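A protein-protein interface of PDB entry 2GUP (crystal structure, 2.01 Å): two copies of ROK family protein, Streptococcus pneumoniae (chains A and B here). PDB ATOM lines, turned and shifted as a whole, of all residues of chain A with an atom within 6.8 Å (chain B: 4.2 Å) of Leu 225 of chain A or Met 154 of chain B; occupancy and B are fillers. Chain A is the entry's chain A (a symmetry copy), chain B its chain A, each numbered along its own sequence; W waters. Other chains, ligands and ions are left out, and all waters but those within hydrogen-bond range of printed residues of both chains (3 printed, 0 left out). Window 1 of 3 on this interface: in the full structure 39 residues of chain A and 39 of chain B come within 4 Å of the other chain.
The backbone carbonyl oxygen (O) of Leu 225 of chain A lies within hydrogen-bond range of the backbone NH (N) of Gly 149 of chain B (2.9 Å). O of Leu 225 of chain A lies close to SD of Met 134 of chain B. The side-chain hydroxyl of Thr 155 of chain B is in hydrogen-bond range of the side-chain amide nitrogen of Gln 217 of chain A, at 2.8 Å. N of Thr 155 of chain B lies within hydrogen-bond range of OD1 of Asn 221 of chain A, 3.1 Å away. N of Thr 155 of chain A lies within hydrogen-bond range of OD1 of Asn 221 of chain B (3.1 Å). The backbone NH (N) of Glu 150 of chain B sits at hydrogen-bond distance from the backbone carbonyl oxygen (O) of Tyr 224 of chain A.
SD of Met 154 of chain A is in hydrogen-bond range of ND2 of Asn 221 of chain A (3.4 Å). The side-chain amide nitrogen (ND2) of Asn 221 of chain B sits at hydrogen-bond distance from the side-chain sulfur (SD) of Met 154 of chain B (3.4 Å). OD1 of Asn 221 of chain A lies close to O of Gln 217 of chain A. The backbone carbonyl oxygen of Met 154 of chain B is in hydrogen-bond range of the backbone NH of Trp 166 of chain B, at 2.6 Å. The side-chain carboxylate of Asp 227 of chain A lies within hydrogen-bond range of the side-chain amide nitrogen of Gln 223 of chain A (3.0 Å).
Among the printed residues, pairs that only touch across the chains: Met 154 of chain A with Asn 221 of chain B, Thr 155 of chain A with Thr 156 of chain B, Asn 221 of chain A with Met 154 of chain B, Tyr 224 of chain A with Tyr 153 of chain B, Leu 225 of chain A with Gly 148 of chain B, Leu 225 of chain A with Glu 150 of chain B, Leu 225 of chain A with Phe 151 of chain B, Leu 225 of chain A with Met 154 of chain B, Asp 227 of chain A with Gly 148 of chain B and Tyr 261 of chain A with Thr 155 of chain B.
Leu 225 of chain A touches six residues of chain B. Met 154 of chain B touches two residues of chain A. Of the printed residues of chain B, Thr 155 of chain A touches Thr 156 (3.9 Å) and Asn 221 (3.1 Å). Of the printed residues of chain B, Asp 227 of chain A touches Gly 148. Gly 218 of chain B touches none of the printed residues of chain A. The nearest printed residue of chain B that does not touch Leu 225 of chain A is Tyr 153 of chain B (4.8 Å). The nearest printed residue of chain B that does not touch Asn 221 of chain A is Tyr 153 of chain B (4.04 Å).
Of the 14 printed residues of chain B, 10 touch a printed residue of chain A. Hydrophobic or aromatic side chains of chain B that line the printed part of chain A: Met 134, Phe 151, Tyr 153 and Met 154. Of the 13 printed residues of chain A, 8 touch a printed residue of chain B. Hydrophobic or aromatic side chains of chain A within 4 Å of the printed part of chain B: Tyr 224, Leu 225 and Tyr 261. Among the printed residues, 16 pairs touch across the chains.
Met 154 of chain A touches Asn 221 of chain B, and with the chains exchanged Asn 221 of chain A touches Met 154 of chain B. Thr 155 of chain A touches Asn 221 of chain B, and with the chains exchanged Asn 221 of chain A touches Thr 155 of chain B.
Water W3 lies within hydrogen-bond range of O of Tyr 153 of chain B (2.6 Å), OH of Tyr 261 of chain A (2.7 Å) and OD1 of Asn 221 of chain A (2.9 Å). Water W1 lies within hydrogen-bond range of OH of Tyr 261 of chain A (2.6 Å), O of Gln 217 of chain A (2.9 Å), OG1 of Thr 155 of chain B (3.0 Å) and OD1 of Asn 221 of chain A (3.4 Å). Water W2 lies within hydrogen-bond range of the side-chain hydroxyl of Thr 155 of chain A (3.0 Å) and the side-chain amide oxygen of Asn 221 of chain B (3.4 Å).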
ATOM      1  N   MET A 154       9.584  13.120  11.269  1.00  0.00           N
ATOM      2  CA  MET A 154       8.392  13.837  10.836  1.00  0.00           C
ATOM      3  C   MET A 154       7.624  14.540  11.990  1.00  0.00           C
ATOM      4  O   MET A 154       7.234  13.916  12.941  1.00  0.00           O
ATOM      5  CB  MET A 154       7.443  12.848  10.179  1.00  0.00           C
ATOM      6  CG  MET A 154       6.173  13.453   9.763  1.00  0.00           C
ATOM      7  SD  MET A 154       5.064  12.153   8.700  1.00  0.00           S
ATOM      8  CE  MET A 154       5.205  10.496   9.815  1.00  0.00           C
ATOM      9  N   THR A 155       7.441  15.833  11.896  1.00  0.00           N
ATOM     10  CA  THR A 155       6.705  16.558  12.945  1.00  0.00           C
ATOM     11  C   THR A 155       5.206  16.598  12.604  1.00  0.00           C
ATOM     12  O   THR A 155       4.766  17.120  11.565  1.00  0.00           O
ATOM     13  CB  THR A 155       7.269  17.975  13.128  1.00  0.00           C
ATOM     14  OG1 THR A 155       7.176  18.686  11.894  1.00  0.00           O
ATOM     15  CG2 THR A 155       8.717  17.935  13.579  1.00  0.00           C
ATOM     16  N   GLN A 217      -1.812   8.776  12.174  1.00  0.00           N
ATOM     17  CA  GLN A 217      -1.771  10.080  11.586  1.00  0.00           C
ATOM     18  C   GLN A 217      -0.524  10.148  10.724  1.00  0.00           C
ATOM     19  O   GLN A 217      -0.534  10.623   9.559  1.00  0.00           O
ATOM     20  CB  GLN A 217      -1.642  11.208  12.676  1.00  0.00           C
ATOM     21  CG  GLN A 217      -1.375  12.538  11.949  1.00  0.00           C
ATOM     22  CD  GLN A 217      -1.075  13.684  12.862  1.00  0.00           C
ATOM     23  OE1 GLN A 217      -1.165  13.580  14.107  1.00  0.00           O
ATOM     24  NE2 GLN A 217      -0.632  14.772  12.276  1.00  0.00           N
ATOM     25  N   LEU A 220      -0.790   7.628   7.368  1.00  0.00           N
ATOM     26  CA  LEU A 220      -1.478   8.364   6.315  1.00  0.00           C
ATOM     27  C   LEU A 220      -0.599   9.449   5.692  1.00  0.00           C
ATOM     28  O   LEU A 220      -0.750   9.695   4.551  1.00  0.00           O
ATOM     29  CB  LEU A 220      -2.800   8.946   6.822  1.00  0.00           C
ATOM     30  CG  LEU A 220      -3.900   7.930   7.069  1.00  0.00           C
ATOM     31  CD1 LEU A 220      -4.959   8.507   8.093  1.00  0.00           C
ATOM     32  CD2 LEU A 220      -4.626   7.616   5.766  1.00  0.00           C
ATOM     33  N   ASN A 221       0.301  10.087   6.409  1.00  0.00           N
ATOM     34  CA  ASN A 221       1.218  10.999   5.779  1.00  0.00           C
ATOM     35  C   ASN A 221       2.136  10.283   4.800  1.00  0.00           C
ATOM     36  O   ASN A 221       2.378  10.728   3.734  1.00  0.00           O
ATOM     37  CB  ASN A 221       2.028  11.733   6.803  1.00  0.00           C
ATOM     38  CG  ASN A 221       1.244  12.788   7.515  1.00  0.00           C
ATOM     39  OD1 ASN A 221       0.119  13.068   7.198  1.00  0.00           O
ATOM     40  ND2 ASN A 221       1.855  13.378   8.479  1.00  0.00           N
ATOM     41  N   ILE A 222       2.612   9.141   5.211  1.00  0.00           N
ATOM     42  CA  ILE A 222       3.586   8.360   4.446  1.00  0.00           C
ATOM     43  C   ILE A 222       2.839   7.930   3.179  1.00  0.00           C
ATOM     44  O   ILE A 222       3.336   8.105   2.155  1.00  0.00           O
ATOM     45  CB  ILE A 222       4.075   7.167   5.299  1.00  0.00           C
ATOM     46  CG1 ILE A 222       5.028   7.699   6.390  1.00  0.00           C
ATOM     47  CG2 ILE A 222       4.886   6.165   4.535  1.00  0.00           C
ATOM     48  CD1 ILE A 222       5.248   6.617   7.532  1.00  0.00           C
ATOM     49  N   GLN A 223       1.637   7.386   3.298  1.00  0.00           N
ATOM     50  CA  GLN A 223       0.802   6.950   2.193  1.00  0.00           C
ATOM     51  C   GLN A 223       0.590   8.064   1.206  1.00  0.00           C
ATOM     52  O   GLN A 223       0.763   7.850  -0.011  1.00  0.00           O
ATOM     53  CB  GLN A 223      -0.590   6.431   2.653  1.00  0.00           C
ATOM     54  CG  GLN A 223      -1.358   5.716   1.483  1.00  0.00           C
ATOM     55  CD  GLN A 223      -0.556   4.520   1.018  1.00  0.00           C
ATOM     56  OE1 GLN A 223      -0.046   3.789   1.865  1.00  0.00           O
ATOM     57  NE2 GLN A 223      -0.339   4.370  -0.297  1.00  0.00           N
ATOM     58  N   TYR A 224       0.216   9.254   1.692  1.00  0.00           N
ATOM     59  CA  TYR A 224       0.013  10.338   0.717  1.00  0.00           C
ATOM     60  C   TYR A 224       1.267  11.023   0.261  1.00  0.00           C
ATOM     61  O   TYR A 224       1.217  11.739  -0.729  1.00  0.00           O
ATOM     62  CB  TYR A 224      -1.023  11.370   1.179  1.00  0.00           C
ATOM     63  CG  TYR A 224      -2.413  10.787   1.144  1.00  0.00           C
ATOM     64  CD1 TYR A 224      -3.308  11.083   0.087  1.00  0.00           C
ATOM     65  CD2 TYR A 224      -2.823   9.919   2.110  1.00  0.00           C
ATOM     66  CE1 TYR A 224      -4.615  10.519   0.072  1.00  0.00           C
ATOM     67  CE2 TYR A 224      -4.076   9.363   2.095  1.00  0.00           C
ATOM     68  CZ  TYR A 224      -4.967   9.650   1.066  1.00  0.00           C
ATOM     69  OH  TYR A 224      -6.202   9.020   1.125  1.00  0.00           O
ATOM     70  N   LEU A 225       2.392  10.831   0.923  1.00  0.00           N
ATOM     71  CA  LEU A 225       3.595  11.465   0.428  1.00  0.00           C
ATOM     72  C   LEU A 225       4.411  10.609  -0.511  1.00  0.00           C
ATOM     73  O   LEU A 225       4.924  11.097  -1.501  1.00  0.00           O
ATOM     74  CB  LEU A 225       4.451  12.026   1.545  1.00  0.00           C
ATOM     75  CG  LEU A 225       4.113  13.483   1.828  1.00  0.00           C
ATOM     76  CD1 LEU A 225       2.627  13.628   2.010  1.00  0.00           C
ATOM     77  CD2 LEU A 225       4.829  14.000   3.009  1.00  0.00           C
ATOM     78  N   ILE A 226       4.540   9.333  -0.208  1.00  0.00           N
ATOM     79  CA  ILE A 226       5.358   8.445  -1.134  1.00  0.00           C
ATOM     80  C   ILE A 226       4.545   7.388  -1.856  1.00  0.00           C
ATOM     81  O   ILE A 226       5.049   6.712  -2.803  1.00  0.00           O
ATOM     82  CB  ILE A 226       6.567   7.762  -0.424  1.00  0.00           C
ATOM     83  CG1 ILE A 226       6.121   6.784   0.607  1.00  0.00           C
ATOM     84  CG2 ILE A 226       7.440   8.795   0.266  1.00  0.00           C
ATOM     85  CD1 ILE A 226       7.270   5.857   1.025  1.00  0.00           C
ATOM     86  N   ASP A 227       3.331   7.203  -1.364  1.00  0.00           N
ATOM     87  CA  ASP A 227       2.333   6.318  -1.927  1.00  0.00           C
ATOM     88  C   ASP A 227       2.923   4.889  -2.209  1.00  0.00           C
ATOM     89  O   ASP A 227       3.026   4.483  -3.360  1.00  0.00           O
ATOM     90  CB  ASP A 227       1.743   6.958  -3.217  1.00  0.00           C
ATOM     91  CG  ASP A 227       0.580   6.122  -3.827  1.00  0.00           C
ATOM     92  OD1 ASP A 227      -0.214   5.510  -3.053  1.00  0.00           O
ATOM     93  OD2 ASP A 227       0.523   6.033  -5.083  1.00  0.00           O
ATOM     94  N   PRO A 228       3.300   4.148  -1.132  1.00  0.00           N
ATOM     95  CA  PRO A 228       3.802   2.821  -1.205  1.00  0.00           C
ATOM     96  C   PRO A 228       2.642   1.798  -1.491  1.00  0.00           C
ATOM     97  O   PRO A 228       1.484   2.085  -1.233  1.00  0.00           O
ATOM     98  CB  PRO A 228       4.447   2.643   0.162  1.00  0.00           C
ATOM     99  CG  PRO A 228       3.496   3.424   1.096  1.00  0.00           C
ATOM    100  CD  PRO A 228       3.219   4.632   0.297  1.00  0.00           C
ATOM    101  N   TYR A 261      -9.542  12.077   2.806  1.00  0.00           N
ATOM    102  CA  TYR A 261      -8.985  10.731   2.612  1.00  0.00           C
ATOM    103  C   TYR A 261      -9.807   9.744   1.785  1.00  0.00           C
ATOM    104  O   TYR A 261     -10.956   9.441   2.096  1.00  0.00           O
ATOM    105  CB  TYR A 261      -8.619  10.048   3.941  1.00  0.00           C
ATOM    106  CG  TYR A 261      -7.467  10.701   4.673  1.00  0.00           C
ATOM    107  CD1 TYR A 261      -7.641  11.146   5.982  1.00  0.00           C
ATOM    108  CD2 TYR A 261      -6.203  10.922   4.052  1.00  0.00           C
ATOM    109  CE1 TYR A 261      -6.610  11.768   6.662  1.00  0.00           C
ATOM    110  CE2 TYR A 261      -5.191  11.560   4.740  1.00  0.00           C
ATOM    111  CZ  TYR A 261      -5.411  11.991   6.066  1.00  0.00           C
ATOM    112  OH  TYR A 261      -4.431  12.609   6.866  1.00  0.00           O
ATOM    113  N   MET B 134       7.699  14.044  -6.846  1.00  0.00           N
ATOM    114  CA  MET B 134       9.048  13.482  -6.627  1.00  0.00           C
ATOM    115  C   MET B 134       9.768  12.948  -7.856  1.00  0.00           C
ATOM    116  O   MET B 134       9.207  12.175  -8.572  1.00  0.00           O
ATOM    117  CB  MET B 134       8.909  12.277  -5.682  1.00  0.00           C
ATOM    118  CG  MET B 134       8.498  12.733  -4.314  1.00  0.00           C
ATOM    119  SD  MET B 134       7.885  11.249  -3.190  1.00  0.00           S
ATOM    120  CE  MET B 134       9.403  10.085  -3.302  1.00  0.00           C
ATOM    121  N   GLY B 148       2.133   9.821  -5.620  1.00  0.00           N
ATOM    122  CA  GLY B 148       3.482  10.227  -5.262  1.00  0.00           C
ATOM    123  C   GLY B 148       3.497  11.748  -5.112  1.00  0.00           C
ATOM    124  O   GLY B 148       2.974  12.448  -5.942  1.00  0.00           O
ATOM    125  N   GLY B 149       4.011  12.254  -4.001  1.00  0.00           N
ATOM    126  CA  GLY B 149       4.377  13.669  -3.901  1.00  0.00           C
ATOM    127  C   GLY B 149       3.176  14.555  -3.670  1.00  0.00           C
ATOM    128  O   GLY B 149       3.233  15.758  -3.961  1.00  0.00           O
ATOM    129  N   GLU B 150       2.092  13.987  -3.138  1.00  0.00           N
ATOM    130  CA  GLU B 150       0.943  14.806  -2.762  1.00  0.00           C
ATOM    131  C   GLU B 150       1.244  15.384  -1.405  1.00  0.00           C
ATOM    132  O   GLU B 150       0.570  15.053  -0.409  1.00  0.00           O
ATOM    133  CB  GLU B 150      -0.352  14.002  -2.752  1.00  0.00           C
ATOM    134  CG  GLU B 150      -0.869  13.653  -4.132  1.00  0.00           C
ATOM    135  CD  GLU B 150      -1.523  14.805  -4.860  1.00  0.00           C
ATOM    136  OE1 GLU B 150      -1.531  16.002  -4.391  1.00  0.00           O
ATOM    137  OE2 GLU B 150      -2.048  14.515  -5.946  1.00  0.00           O
ATOM    138  N   PHE B 151       2.276  16.252  -1.378  1.00  0.00           N
ATOM    139  CA  PHE B 151       2.698  16.823  -0.097  1.00  0.00           C
ATOM    140  C   PHE B 151       1.598  17.654   0.555  1.00  0.00           C
ATOM    141  O   PHE B 151       1.641  17.858   1.786  1.00  0.00           O
ATOM    142  CB  PHE B 151       3.804  17.771  -0.358  1.00  0.00           C
ATOM    143  CG  PHE B 151       4.986  17.122  -0.974  1.00  0.00           C
ATOM    144  CD1 PHE B 151       5.505  15.961  -0.419  1.00  0.00           C
ATOM    145  CD2 PHE B 151       5.512  17.618  -2.146  1.00  0.00           C
ATOM    146  CE1 PHE B 151       6.587  15.298  -1.001  1.00  0.00           C
ATOM    147  CE2 PHE B 151       6.655  17.042  -2.662  1.00  0.00           C
ATOM    148  CZ  PHE B 151       7.165  15.848  -2.117  1.00  0.00           C
ATOM    149  N   GLY B 152       0.665  18.185  -0.232  1.00  0.00           N
ATOM    150  CA  GLY B 152      -0.466  18.977   0.435  1.00  0.00           C
ATOM    151  C   GLY B 152      -1.336  18.169   1.347  1.00  0.00           C
ATOM    152  O   GLY B 152      -2.050  18.718   2.212  1.00  0.00           O
ATOM    153  N   TYR B 153      -1.229  16.846   1.268  1.00  0.00           N
ATOM    154  CA  TYR B 153      -2.018  16.012   2.211  1.00  0.00           C
ATOM    155  C   TYR B 153      -1.367  15.817   3.589  1.00  0.00           C
ATOM    156  O   TYR B 153      -1.990  15.217   4.504  1.00  0.00           O
ATOM    157  CB  TYR B 153      -2.288  14.653   1.609  1.00  0.00           C
ATOM    158  CG  TYR B 153      -3.404  14.622   0.595  1.00  0.00           C
ATOM    159  CD1 TYR B 153      -3.177  14.965  -0.723  1.00  0.00           C
ATOM    160  CD2 TYR B 153      -4.688  14.169   0.960  1.00  0.00           C
ATOM    161  CE1 TYR B 153      -4.219  14.895  -1.680  1.00  0.00           C
ATOM    162  CE2 TYR B 153      -5.721  14.076   0.026  1.00  0.00           C
ATOM    163  CZ  TYR B 153      -5.478  14.444  -1.291  1.00  0.00           C
ATOM    164  OH  TYR B 153      -6.515  14.384  -2.178  1.00  0.00           O
ATOM    165  N   MET B 154      -0.118  16.230   3.738  1.00  0.00           N
ATOM    166  CA  MET B 154       0.609  16.034   4.986  1.00  0.00           C
ATOM    167  C   MET B 154       0.034  16.838   6.185  1.00  0.00           C
ATOM    168  O   MET B 154      -0.085  18.033   6.125  1.00  0.00           O
ATOM    169  CB  MET B 154       2.050  16.471   4.779  1.00  0.00           C
ATOM    170  CG  MET B 154       2.862  16.380   5.998  1.00  0.00           C
ATOM    171  SD  MET B 154       4.802  16.748   5.607  1.00  0.00           S
ATOM    172  CE  MET B 154       4.678  18.384   4.461  1.00  0.00           C
ATOM    173  N   THR B 155      -0.335  16.164   7.245  1.00  0.00           N
ATOM    174  CA  THR B 155      -0.870  16.866   8.423  1.00  0.00           C
ATOM    175  C   THR B 155       0.274  17.225   9.387  1.00  0.00           C
ATOM    176  O   THR B 155       1.011  16.368   9.903  1.00  0.00           O
ATOM    177  CB  THR B 155      -1.940  16.017   9.125  1.00  0.00           C
ATOM    178  OG1 THR B 155      -1.370  14.770   9.525  1.00  0.00           O
ATOM    179  CG2 THR B 155      -3.124  15.760   8.213  1.00  0.00           C
ATOM    180  N   THR B 156       0.443  18.506   9.586  1.00  0.00           N
ATOM    181  CA  THR B 156       1.517  19.045  10.436  1.00  0.00           C
ATOM    182  C   THR B 156       0.957  19.537  11.749  1.00  0.00           C
ATOM    183  O   THR B 156       1.680  20.126  12.544  1.00  0.00           O
ATOM    184  CB  THR B 156       2.145  20.236   9.769  1.00  0.00           C
ATOM    185  OG1 THR B 156       1.095  21.156   9.385  1.00  0.00           O
ATOM    186  CG2 THR B 156       2.921  19.795   8.595  1.00  0.00           C
ATOM    187  N   ASN B 165      -4.242  19.544   7.107  1.00  0.00           N
ATOM    188  CA  ASN B 165      -3.212  19.187   6.109  1.00  0.00           C
ATOM    189  C   ASN B 165      -2.436  20.430   5.646  1.00  0.00           C
ATOM    190  O   ASN B 165      -2.921  21.610   5.755  1.00  0.00           O
ATOM    191  CB  ASN B 165      -3.821  18.390   4.905  1.00  0.00           C
ATOM    192  CG  ASN B 165      -4.953  19.156   4.183  1.00  0.00           C
ATOM    193  OD1 ASN B 165      -5.862  19.637   4.831  1.00  0.00           O
ATOM    194  ND2 ASN B 165      -4.918  19.236   2.852  1.00  0.00           N
ATOM    195  N   TRP B 166      -1.195  20.204   5.169  1.00  0.00           N
ATOM    196  CA  TRP B 166      -0.312  21.254   4.709  1.00  0.00           C
ATOM    197  C   TRP B 166      -0.955  22.252   3.742  1.00  0.00           C
ATOM    198  O   TRP B 166      -0.776  23.463   3.921  1.00  0.00           O
ATOM    199  CB  TRP B 166       0.964  20.649   4.107  1.00  0.00           C
ATOM    200  CG  TRP B 166       2.235  21.509   4.286  1.00  0.00           C
ATOM    201  CD1 TRP B 166       2.595  22.368   5.369  1.00  0.00           C
ATOM    202  CD2 TRP B 166       3.305  21.483   3.399  1.00  0.00           C
ATOM    203  NE1 TRP B 166       3.838  22.868   5.104  1.00  0.00           N
ATOM    204  CE2 TRP B 166       4.305  22.319   3.908  1.00  0.00           C
ATOM    205  CE3 TRP B 166       3.503  20.824   2.133  1.00  0.00           C
ATOM    206  CZ2 TRP B 166       5.518  22.554   3.205  1.00  0.00           C
ATOM    207  CZ3 TRP B 166       4.744  20.979   1.478  1.00  0.00           C
ATOM    208  CH2 TRP B 166       5.726  21.856   2.018  1.00  0.00           C
ATOM    209  N   GLY B 218       6.976  21.897   7.118  1.00  0.00           N
ATOM    210  CA  GLY B 218       6.630  20.847   6.216  1.00  0.00           C
ATOM    211  C   GLY B 218       7.844  20.544   5.297  1.00  0.00           C
ATOM    212  O   GLY B 218       8.069  19.416   4.961  1.00  0.00           O
ATOM    213  N   ASN B 221      10.153  18.153   6.866  1.00  0.00           N
ATOM    214  CA  ASN B 221       9.611  16.820   6.840  1.00  0.00           C
ATOM    215  C   ASN B 221       9.982  16.089   5.559  1.00  0.00           C
ATOM    216  O   ASN B 221      10.345  14.966   5.567  1.00  0.00           O
ATOM    217  CB  ASN B 221       8.123  16.848   7.005  1.00  0.00           C
ATOM    218  CG  ASN B 221       7.700  17.147   8.408  1.00  0.00           C
ATOM    219  OD1 ASN B 221       8.493  17.239   9.306  1.00  0.00           O
ATOM    220  ND2 ASN B 221       6.435  17.290   8.588  1.00  0.00           N
HETATM  221  O   HOH W   1      -2.786  12.245   8.862  1.00  0.00           O
HETATM  222  O   HOH W   2       9.560  20.125  10.861  1.00  0.00           O
HETATM  223  O   HOH W   3      -2.191  12.815   5.406  1.00  0.00           O
